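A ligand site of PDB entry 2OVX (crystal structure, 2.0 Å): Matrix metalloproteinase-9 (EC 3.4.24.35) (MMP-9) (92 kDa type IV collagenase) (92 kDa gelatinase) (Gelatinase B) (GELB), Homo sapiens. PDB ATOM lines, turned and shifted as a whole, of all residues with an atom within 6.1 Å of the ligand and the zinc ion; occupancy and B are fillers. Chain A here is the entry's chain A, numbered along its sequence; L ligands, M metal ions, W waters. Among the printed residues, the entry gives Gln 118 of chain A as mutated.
Within 4 Å of the zinc ion: His 117, His 121 and His 127.
The backbone NH (N) of Ala 80 is in hydrogen-bond range of an oxygen (O4) of the ligand, at 3.4 Å.
A nitrogen (N2) of the ligand sits at hydrogen-bond distance from the backbone carbonyl oxygen (O) of Ala 80, 2.7 Å away.
The backbone NH (N) of Leu 79 is in hydrogen-bond range of an oxygen (O4) of the ligand, 2.9 Å away.
The side-chain amide nitrogen (NE2) of Gln 118 sits at hydrogen-bond distance from an oxygen (O3) of the ligand (3.2 Å).
Water W2 bridges O3 of the ligand and N of Ala 82.
Merely in contact with the ligand: Pro 137 (3.1 Å), Leu 134 (3.2 Å), Arg 140 (3.3 Å), Tyr 139 (3.4 Å), Tyr 136 (3.5 Å), Met 138 (3.5 Å), Leu 78 (3.7 Å), Gly 77 (3.7 Å), Val 114 (3.9 Å) and His 81 (3.9 Å).
Hydrophobic or aromatic side chains within 4 Å of the ligand: Leu 78, Leu 79, Val 114, His 117, His 121, His 127, Pro 137 and Tyr 139.
Within 4 Å of the ligand: Gly 77, Leu 78, Leu 79, Ala 80, His 81, Val 114, His 117, Gln 118, His 121, His 127, Leu 134, Tyr 136, Pro 137, Met 138, Tyr 139 and Arg 140.
NE2 of His 121 is bound to the zinc ion, 2.0 Å away.
N1 of the ligand binds the zinc ion (2.0 Å).
A ring nitrogen (NE2) of His 117 is bound to the zinc ion.
The zinc ion is bound by a ring nitrogen (NE2) of His 127.
A ring nitrogen (ND1) of His 117 is in hydrogen-bond range of the backbone carbonyl oxygen (O) of Leu 134, at 2.7 Å.
The side-chain amide nitrogen (NE2) of Gln 118 sits close to the backbone NH (N) of Ala 82.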
ATOM      1  N   ASP A  76      -8.791   0.288 -20.498  1.00  0.00           N
ATOM      2  CA  ASP A  76      -9.414  -0.980 -20.153  1.00  0.00           C
ATOM      3  C   ASP A  76      -9.266  -1.391 -18.695  1.00  0.00           C
ATOM      4  O   ASP A  76      -8.918  -0.582 -17.842  1.00  0.00           O
ATOM      5  CB  ASP A  76      -8.871  -2.099 -21.054  1.00  0.00           C
ATOM      6  CG  ASP A  76      -9.209  -1.875 -22.517  1.00  0.00           C
ATOM      7  OD1 ASP A  76     -10.412  -1.795 -22.849  1.00  0.00           O
ATOM      8  OD2 ASP A  76      -8.275  -1.771 -23.339  1.00  0.00           O
ATOM      9  N   GLY A  77      -9.519  -2.671 -18.417  1.00  0.00           N
ATOM     10  CA  GLY A  77      -9.425  -3.134 -17.047  1.00  0.00           C
ATOM     11  C   GLY A  77     -10.515  -2.474 -16.224  1.00  0.00           C
ATOM     12  O   GLY A  77     -11.678  -2.475 -16.610  1.00  0.00           O
ATOM     13  N   LEU A  78     -10.148  -1.892 -15.083  1.00  0.00           N
ATOM     14  CA  LEU A  78     -11.107  -1.203 -14.233  1.00  0.00           C
ATOM     15  C   LEU A  78     -11.650  -0.013 -15.019  1.00  0.00           C
ATOM     16  O   LEU A  78     -10.892   0.829 -15.495  1.00  0.00           O
ATOM     17  CB  LEU A  78     -10.424  -0.720 -12.948  1.00  0.00           C
ATOM     18  CG  LEU A  78     -11.297  -0.005 -11.909  1.00  0.00           C
ATOM     19  CD1 LEU A  78     -12.459  -0.886 -11.522  1.00  0.00           C
ATOM     20  CD2 LEU A  78     -10.452   0.339 -10.687  1.00  0.00           C
ATOM     21  N   LEU A  79     -12.978   0.056 -15.158  1.00  0.00           N
ATOM     22  CA  LEU A  79     -13.610   1.120 -15.919  1.00  0.00           C
ATOM     23  C   LEU A  79     -14.020   2.291 -15.033  1.00  0.00           C
ATOM     24  O   LEU A  79     -14.053   3.439 -15.485  1.00  0.00           O
ATOM     25  CB  LEU A  79     -14.838   0.589 -16.659  1.00  0.00           C
ATOM     26  CG  LEU A  79     -14.639  -0.647 -17.553  1.00  0.00           C
ATOM     27  CD1 LEU A  79     -15.984  -1.108 -18.104  1.00  0.00           C
ATOM     28  CD2 LEU A  79     -13.685  -0.298 -18.684  1.00  0.00           C
ATOM     29  N   ALA A  80     -14.329   1.982 -13.778  1.00  0.00           N
ATOM     30  CA  ALA A  80     -14.762   2.981 -12.819  1.00  0.00           C
ATOM     31  C   ALA A  80     -15.058   2.286 -11.500  1.00  0.00           C
ATOM     32  O   ALA A  80     -14.891   1.074 -11.375  1.00  0.00           O
ATOM     33  CB  ALA A  80     -16.024   3.665 -13.326  1.00  0.00           C
ATOM     34  N   HIS A  81     -15.485   3.062 -10.515  1.00  0.00           N
ATOM     35  CA  HIS A  81     -15.876   2.497  -9.227  1.00  0.00           C
ATOM     36  C   HIS A  81     -16.742   3.485  -8.479  1.00  0.00           C
ATOM     37  O   HIS A  81     -16.681   4.697  -8.718  1.00  0.00           O
ATOM     38  CB  HIS A  81     -14.635   2.079  -8.407  1.00  0.00           C
ATOM     39  CG  HIS A  81     -13.664   3.182  -8.124  1.00  0.00           C
ATOM     40  ND1 HIS A  81     -12.313   2.949  -7.964  1.00  0.00           N
ATOM     41  CD2 HIS A  81     -13.833   4.510  -7.935  1.00  0.00           C
ATOM     42  CE1 HIS A  81     -11.693   4.076  -7.682  1.00  0.00           C
ATOM     43  NE2 HIS A  81     -12.598   5.042  -7.649  1.00  0.00           N
ATOM     44  N   ALA A  82     -17.590   2.971  -7.604  1.00  0.00           N
ATOM     45  CA  ALA A  82     -18.479   3.830  -6.845  1.00  0.00           C
ATOM     46  C   ALA A  82     -18.590   3.329  -5.418  1.00  0.00           C
ATOM     47  O   ALA A  82     -18.640   2.126  -5.176  1.00  0.00           O
ATOM     48  CB  ALA A  82     -19.860   3.858  -7.496  1.00  0.00           C
ATOM     49  N   LEU A 113     -24.349   2.979 -19.962  1.00  0.00           N
ATOM     50  CA  LEU A 113     -24.439   1.689 -19.288  1.00  0.00           C
ATOM     51  C   LEU A 113     -23.511   1.587 -18.088  1.00  0.00           C
ATOM     52  O   LEU A 113     -23.925   1.095 -17.042  1.00  0.00           O
ATOM     53  CB  LEU A 113     -24.137   0.550 -20.265  1.00  0.00           C
ATOM     54  CG  LEU A 113     -25.147   0.354 -21.403  1.00  0.00           C
ATOM     55  CD1 LEU A 113     -24.666  -0.780 -22.311  1.00  0.00           C
ATOM     56  CD2 LEU A 113     -26.512   0.021 -20.827  1.00  0.00           C
ATOM     57  N   VAL A 114     -22.273   2.039 -18.228  1.00  0.00           N
ATOM     58  CA  VAL A 114     -21.330   1.970 -17.116  1.00  0.00           C
ATOM     59  C   VAL A 114     -21.839   2.833 -15.954  1.00  0.00           C
ATOM     60  O   VAL A 114     -21.781   2.403 -14.790  1.00  0.00           O
ATOM     61  CB  VAL A 114     -19.900   2.422 -17.546  1.00  0.00           C
ATOM     62  CG1 VAL A 114     -18.971   2.450 -16.352  1.00  0.00           C
ATOM     63  CG2 VAL A 114     -19.341   1.439 -18.584  1.00  0.00           C
ATOM     64  N   ALA A 115     -22.336   4.026 -16.250  1.00  0.00           N
ATOM     65  CA  ALA A 115     -22.847   4.905 -15.192  1.00  0.00           C
ATOM     66  C   ALA A 115     -24.032   4.223 -14.505  1.00  0.00           C
ATOM     67  O   ALA A 115     -24.112   4.220 -13.273  1.00  0.00           O
ATOM     68  CB  ALA A 115     -23.265   6.257 -15.774  1.00  0.00           C
ATOM     69  N   HIS A 117     -24.615   1.173 -14.087  1.00  0.00           N
ATOM     70  CA  HIS A 117     -24.063   0.119 -13.212  1.00  0.00           C
ATOM     71  C   HIS A 117     -23.464   0.750 -11.955  1.00  0.00           C
ATOM     72  O   HIS A 117     -23.749   0.305 -10.832  1.00  0.00           O
ATOM     73  CB  HIS A 117     -22.978  -0.653 -13.978  1.00  0.00           C
ATOM     74  CG  HIS A 117     -22.328  -1.731 -13.170  1.00  0.00           C
ATOM     75  ND1 HIS A 117     -22.722  -3.055 -13.232  1.00  0.00           N
ATOM     76  CD2 HIS A 117     -21.293  -1.695 -12.289  1.00  0.00           C
ATOM     77  CE1 HIS A 117     -21.957  -3.779 -12.435  1.00  0.00           C
ATOM     78  NE2 HIS A 117     -21.079  -2.975 -11.854  1.00  0.00           N
ATOM     79  N   GLN A 118     -22.635   1.774 -12.137  1.00  0.00           N
ATOM     80  CA  GLN A 118     -21.996   2.459 -11.013  1.00  0.00           C
ATOM     81  C   GLN A 118     -23.020   3.077 -10.059  1.00  0.00           C
ATOM     82  O   GLN A 118     -22.825   3.076  -8.846  1.00  0.00           O
ATOM     83  CB  GLN A 118     -21.049   3.569 -11.492  1.00  0.00           C
ATOM     84  CG  GLN A 118     -19.920   3.102 -12.403  1.00  0.00           C
ATOM     85  CD  GLN A 118     -19.226   1.855 -11.890  1.00  0.00           C
ATOM     86  OE1 GLN A 118     -19.040   0.892 -12.613  1.00  0.00           O
ATOM     87  NE2 GLN A 118     -18.826   1.887 -10.620  1.00  0.00           N
ATOM     88  N   HIS A 121     -24.243   0.611  -7.683  1.00  0.00           N
ATOM     89  CA  HIS A 121     -23.329   0.484  -6.559  1.00  0.00           C
ATOM     90  C   HIS A 121     -23.524   1.655  -5.583  1.00  0.00           C
ATOM     91  O   HIS A 121     -23.583   1.461  -4.372  1.00  0.00           O
ATOM     92  CB  HIS A 121     -21.861   0.504  -7.033  1.00  0.00           C
ATOM     93  CG  HIS A 121     -21.406  -0.785  -7.621  1.00  0.00           C
ATOM     94  ND1 HIS A 121     -21.562  -1.988  -6.983  1.00  0.00           N
ATOM     95  CD2 HIS A 121     -20.736  -1.058  -8.774  1.00  0.00           C
ATOM     96  CE1 HIS A 121     -21.033  -2.955  -7.707  1.00  0.00           C
ATOM     97  NE2 HIS A 121     -20.518  -2.417  -8.806  1.00  0.00           N
ATOM     98  N   HIS A 127     -22.842  -6.821  -6.876  1.00  0.00           N
ATOM     99  CA  HIS A 127     -22.860  -7.461  -8.173  1.00  0.00           C
ATOM    100  C   HIS A 127     -23.928  -8.547  -8.244  1.00  0.00           C
ATOM    101  O   HIS A 127     -24.311  -9.120  -7.223  1.00  0.00           O
ATOM    102  CB  HIS A 127     -21.486  -8.044  -8.483  1.00  0.00           C
ATOM    103  CG  HIS A 127     -20.481  -7.013  -8.856  1.00  0.00           C
ATOM    104  ND1 HIS A 127     -19.122  -7.188  -8.671  1.00  0.00           N
ATOM    105  CD2 HIS A 127     -20.631  -5.791  -9.431  1.00  0.00           C
ATOM    106  CE1 HIS A 127     -18.478  -6.118  -9.119  1.00  0.00           C
ATOM    107  NE2 HIS A 127     -19.373  -5.260  -9.584  1.00  0.00           N
ATOM    108  N   ALA A 133     -27.937  -9.417 -16.322  1.00  0.00           N
ATOM    109  CA  ALA A 133     -28.282  -8.268 -15.491  1.00  0.00           C
ATOM    110  C   ALA A 133     -27.282  -7.118 -15.613  1.00  0.00           C
ATOM    111  O   ALA A 133     -26.116  -7.335 -15.927  1.00  0.00           O
ATOM    112  CB  ALA A 133     -28.396  -8.701 -14.032  1.00  0.00           C
ATOM    113  N   LEU A 134     -27.747  -5.903 -15.362  1.00  0.00           N
ATOM    114  CA  LEU A 134     -26.872  -4.726 -15.434  1.00  0.00           C
ATOM    115  C   LEU A 134     -25.784  -4.784 -14.355  1.00  0.00           C
ATOM    116  O   LEU A 134     -24.659  -4.330 -14.578  1.00  0.00           O
ATOM    117  CB  LEU A 134     -27.693  -3.442 -15.267  1.00  0.00           C
ATOM    118  CG  LEU A 134     -26.921  -2.127 -15.145  1.00  0.00           C
ATOM    119  CD1 LEU A 134     -26.158  -1.839 -16.433  1.00  0.00           C
ATOM    120  CD2 LEU A 134     -27.890  -0.989 -14.856  1.00  0.00           C
ATOM    121  N   MET A 135     -26.119  -5.347 -13.198  1.00  0.00           N
ATOM    122  CA  MET A 135     -25.150  -5.437 -12.110  1.00  0.00           C
ATOM    123  C   MET A 135     -24.142  -6.576 -12.234  1.00  0.00           C
ATOM    124  O   MET A 135     -23.376  -6.844 -11.299  1.00  0.00           O
ATOM    125  CB  MET A 135     -25.868  -5.491 -10.761  1.00  0.00           C
ATOM    126  CG  MET A 135     -26.637  -4.218 -10.445  1.00  0.00           C
ATOM    127  SD  MET A 135     -25.661  -2.706 -10.750  1.00  0.00           S
ATOM    128  CE  MET A 135     -24.427  -2.792  -9.488  1.00  0.00           C
ATOM    129  N   TYR A 136     -24.131  -7.254 -13.380  1.00  0.00           N
ATOM    130  CA  TYR A 136     -23.181  -8.343 -13.621  1.00  0.00           C
ATOM    131  C   TYR A 136     -21.831  -7.641 -13.910  1.00  0.00           C
ATOM    132  O   TYR A 136     -21.755  -6.773 -14.777  1.00  0.00           O
ATOM    133  CB  TYR A 136     -23.631  -9.167 -14.833  1.00  0.00           C
ATOM    134  CG  TYR A 136     -22.769 -10.378 -15.133  1.00  0.00           C
ATOM    135  CD1 TYR A 136     -22.656 -11.423 -14.210  1.00  0.00           C
ATOM    136  CD2 TYR A 136     -22.082 -10.489 -16.339  1.00  0.00           C
ATOM    137  CE1 TYR A 136     -21.866 -12.549 -14.485  1.00  0.00           C
ATOM    138  CE2 TYR A 136     -21.299 -11.614 -16.626  1.00  0.00           C
ATOM    139  CZ  TYR A 136     -21.196 -12.639 -15.696  1.00  0.00           C
ATOM    140  OH  TYR A 136     -20.402 -13.735 -15.979  1.00  0.00           O
ATOM    141  N   PRO A 137     -20.760  -8.022 -13.177  1.00  0.00           N
ATOM    142  CA  PRO A 137     -19.422  -7.436 -13.338  1.00  0.00           C
ATOM    143  C   PRO A 137     -18.671  -7.749 -14.616  1.00  0.00           C
ATOM    144  O   PRO A 137     -17.552  -8.252 -14.567  1.00  0.00           O
ATOM    145  CB  PRO A 137     -18.695  -7.948 -12.100  1.00  0.00           C
ATOM    146  CG  PRO A 137     -19.264  -9.320 -11.951  1.00  0.00           C
ATOM    147  CD  PRO A 137     -20.747  -9.086 -12.157  1.00  0.00           C
ATOM    148  N   MET A 138     -19.265  -7.433 -15.751  1.00  0.00           N
ATOM    149  CA  MET A 138     -18.647  -7.675 -17.052  1.00  0.00           C
ATOM    150  C   MET A 138     -19.257  -6.770 -18.103  1.00  0.00           C
ATOM    151  O   MET A 138     -20.463  -6.814 -18.346  1.00  0.00           O
ATOM    152  CB  MET A 138     -18.881  -9.135 -17.447  1.00  0.00           C
ATOM    153  CG  MET A 138     -17.633  -9.986 -17.446  1.00  0.00           C
ATOM    154  SD  MET A 138     -16.475  -9.465 -18.704  1.00  0.00           S
ATOM    155  CE  MET A 138     -17.456  -9.778 -20.180  1.00  0.00           C
ATOM    156  N   TYR A 139     -18.437  -5.944 -18.739  1.00  0.00           N
ATOM    157  CA  TYR A 139     -18.961  -5.045 -19.766  1.00  0.00           C
ATOM    158  C   TYR A 139     -19.269  -5.744 -21.081  1.00  0.00           C
ATOM    159  O   TYR A 139     -18.413  -6.409 -21.657  1.00  0.00           O
ATOM    160  CB  TYR A 139     -17.998  -3.885 -20.053  1.00  0.00           C
ATOM    161  CG  TYR A 139     -18.598  -2.883 -21.036  1.00  0.00           C
ATOM    162  CD1 TYR A 139     -19.409  -1.843 -20.592  1.00  0.00           C
ATOM    163  CD2 TYR A 139     -18.419  -3.030 -22.411  1.00  0.00           C
ATOM    164  CE1 TYR A 139     -20.031  -0.974 -21.492  1.00  0.00           C
ATOM    165  CE2 TYR A 139     -19.030  -2.172 -23.318  1.00  0.00           C
ATOM    166  CZ  TYR A 139     -19.838  -1.154 -22.854  1.00  0.00           C
ATOM    167  OH  TYR A 139     -20.486  -0.333 -23.751  1.00  0.00           O
ATOM    168  N   ARG A 140     -20.494  -5.586 -21.541  1.00  0.00           N
ATOM    169  CA  ARG A 140     -20.930  -6.157 -22.805  1.00  0.00           C
ATOM    170  C   ARG A 140     -22.029  -5.234 -23.302  1.00  0.00           C
ATOM    171  O   ARG A 140     -22.996  -4.969 -22.592  1.00  0.00           O
ATOM    172  CB  ARG A 140     -21.505  -7.572 -22.607  1.00  0.00           C
ATOM    173  N   PHE A 141     -21.871  -4.716 -24.509  1.00  0.00           N
ATOM    174  CA  PHE A 141     -22.920  -3.845 -25.016  1.00  0.00           C
ATOM    175  C   PHE A 141     -23.998  -4.650 -25.702  1.00  0.00           C
ATOM    176  O   PHE A 141     -23.716  -5.524 -26.522  1.00  0.00           O
ATOM    177  CB  PHE A 141     -22.384  -2.812 -26.002  1.00  0.00           C
ATOM    178  CG  PHE A 141     -23.468  -1.974 -26.622  1.00  0.00           C
ATOM    179  CD1 PHE A 141     -24.211  -2.464 -27.686  1.00  0.00           C
ATOM    180  CD2 PHE A 141     -23.800  -0.742 -26.086  1.00  0.00           C
ATOM    181  CE1 PHE A 141     -25.277  -1.741 -28.212  1.00  0.00           C
ATOM    182  CE2 PHE A 141     -24.868  -0.010 -26.601  1.00  0.00           C
ATOM    183  CZ  PHE A 141     -25.605  -0.511 -27.654  1.00  0.00           C
HETATM  184  C1  LIG L   1     -22.333  -4.016 -16.812  1.00  0.00           C
HETATM  185  C2  LIG L   1     -23.227  -4.942 -17.328  1.00  0.00           C
HETATM  186  C3  LIG L   1     -23.632  -4.840 -18.657  1.00  0.00           C
HETATM  187  C4  LIG L   1     -23.135  -3.833 -19.468  1.00  0.00           C
HETATM  188  C5  LIG L   1     -22.221  -2.908 -18.946  1.00  0.00           C
HETATM  189  C6  LIG L   1     -21.827  -2.990 -17.609  1.00  0.00           C
HETATM  190  O1  LIG L   1     -21.116  -1.961 -17.077  1.00  0.00           O
HETATM  191  C7  LIG L   1     -20.085  -2.263 -16.249  1.00  0.00           C
HETATM  192  C8  LIG L   1     -19.616  -1.263 -15.400  1.00  0.00           C
HETATM  193  C9  LIG L   1     -18.481  -1.470 -14.623  1.00  0.00           C
HETATM  194  C10 LIG L   1     -19.386  -3.463 -16.323  1.00  0.00           C
HETATM  195  C11 LIG L   1     -18.250  -3.670 -15.546  1.00  0.00           C
HETATM  196  C12 LIG L   1     -17.797  -2.679 -14.680  1.00  0.00           C
HETATM  197  C13 LIG L   1     -16.795  -3.043 -13.571  1.00  0.00           C
HETATM  198  C14 LIG L   1     -17.645  -3.570 -12.417  1.00  0.00           C
HETATM  199  O2  LIG L   1     -18.105  -4.719 -12.491  1.00  0.00           O
HETATM  200  N1  LIG L   1     -17.839  -2.850 -11.236  1.00  0.00           N
HETATM  201  C15 LIG L   1     -17.202  -1.611 -11.018  1.00  0.00           C
HETATM  202  O3  LIG L   1     -17.529  -0.931 -10.051  1.00  0.00           O
HETATM  203  N2  LIG L   1     -16.321  -1.095 -11.978  1.00  0.00           N
HETATM  204  C16 LIG L   1     -16.012  -1.793 -13.158  1.00  0.00           C
HETATM  205  O4  LIG L   1     -15.217  -1.289 -13.955  1.00  0.00           O
HETATM  206  N3  LIG L   1     -15.888  -4.109 -14.031  1.00  0.00           N
HETATM  207  C17 LIG L   1     -15.127  -3.733 -15.245  1.00  0.00           C
HETATM  208  C18 LIG L   1     -14.325  -4.939 -15.747  1.00  0.00           C
HETATM  209  C19 LIG L   1     -14.985  -4.584 -12.972  1.00  0.00           C
HETATM  210  C20 LIG L   1     -14.162  -5.782 -13.468  1.00  0.00           C
HETATM  211  N4  LIG L   1     -13.424  -5.375 -14.667  1.00  0.00           N
HETATM  212  C21 LIG L   1     -12.421  -6.348 -15.108  1.00  0.00           C
HETATM  213  N5  LIG L   1     -11.857  -6.209 -16.320  1.00  0.00           N
HETATM  214  C22 LIG L   1     -10.742  -6.844 -16.649  1.00  0.00           C
HETATM  215  C23 LIG L   1     -10.133  -7.683 -15.731  1.00  0.00           C
HETATM  216  C24 LIG L   1     -10.747  -7.839 -14.492  1.00  0.00           C
HETATM  217  N6  LIG L   1     -11.857  -7.183 -14.213  1.00  0.00           N
HETATM  218 ZN    ZN M   1     -19.619  -3.248 -10.370  1.00  0.00          ZN
HETATM  219  O   HOH W   1     -15.482  -5.751 -18.506  1.00  0.00           O
HETATM  220  O   HOH W   2     -17.389  -0.004  -7.604  1.00  0.00           O
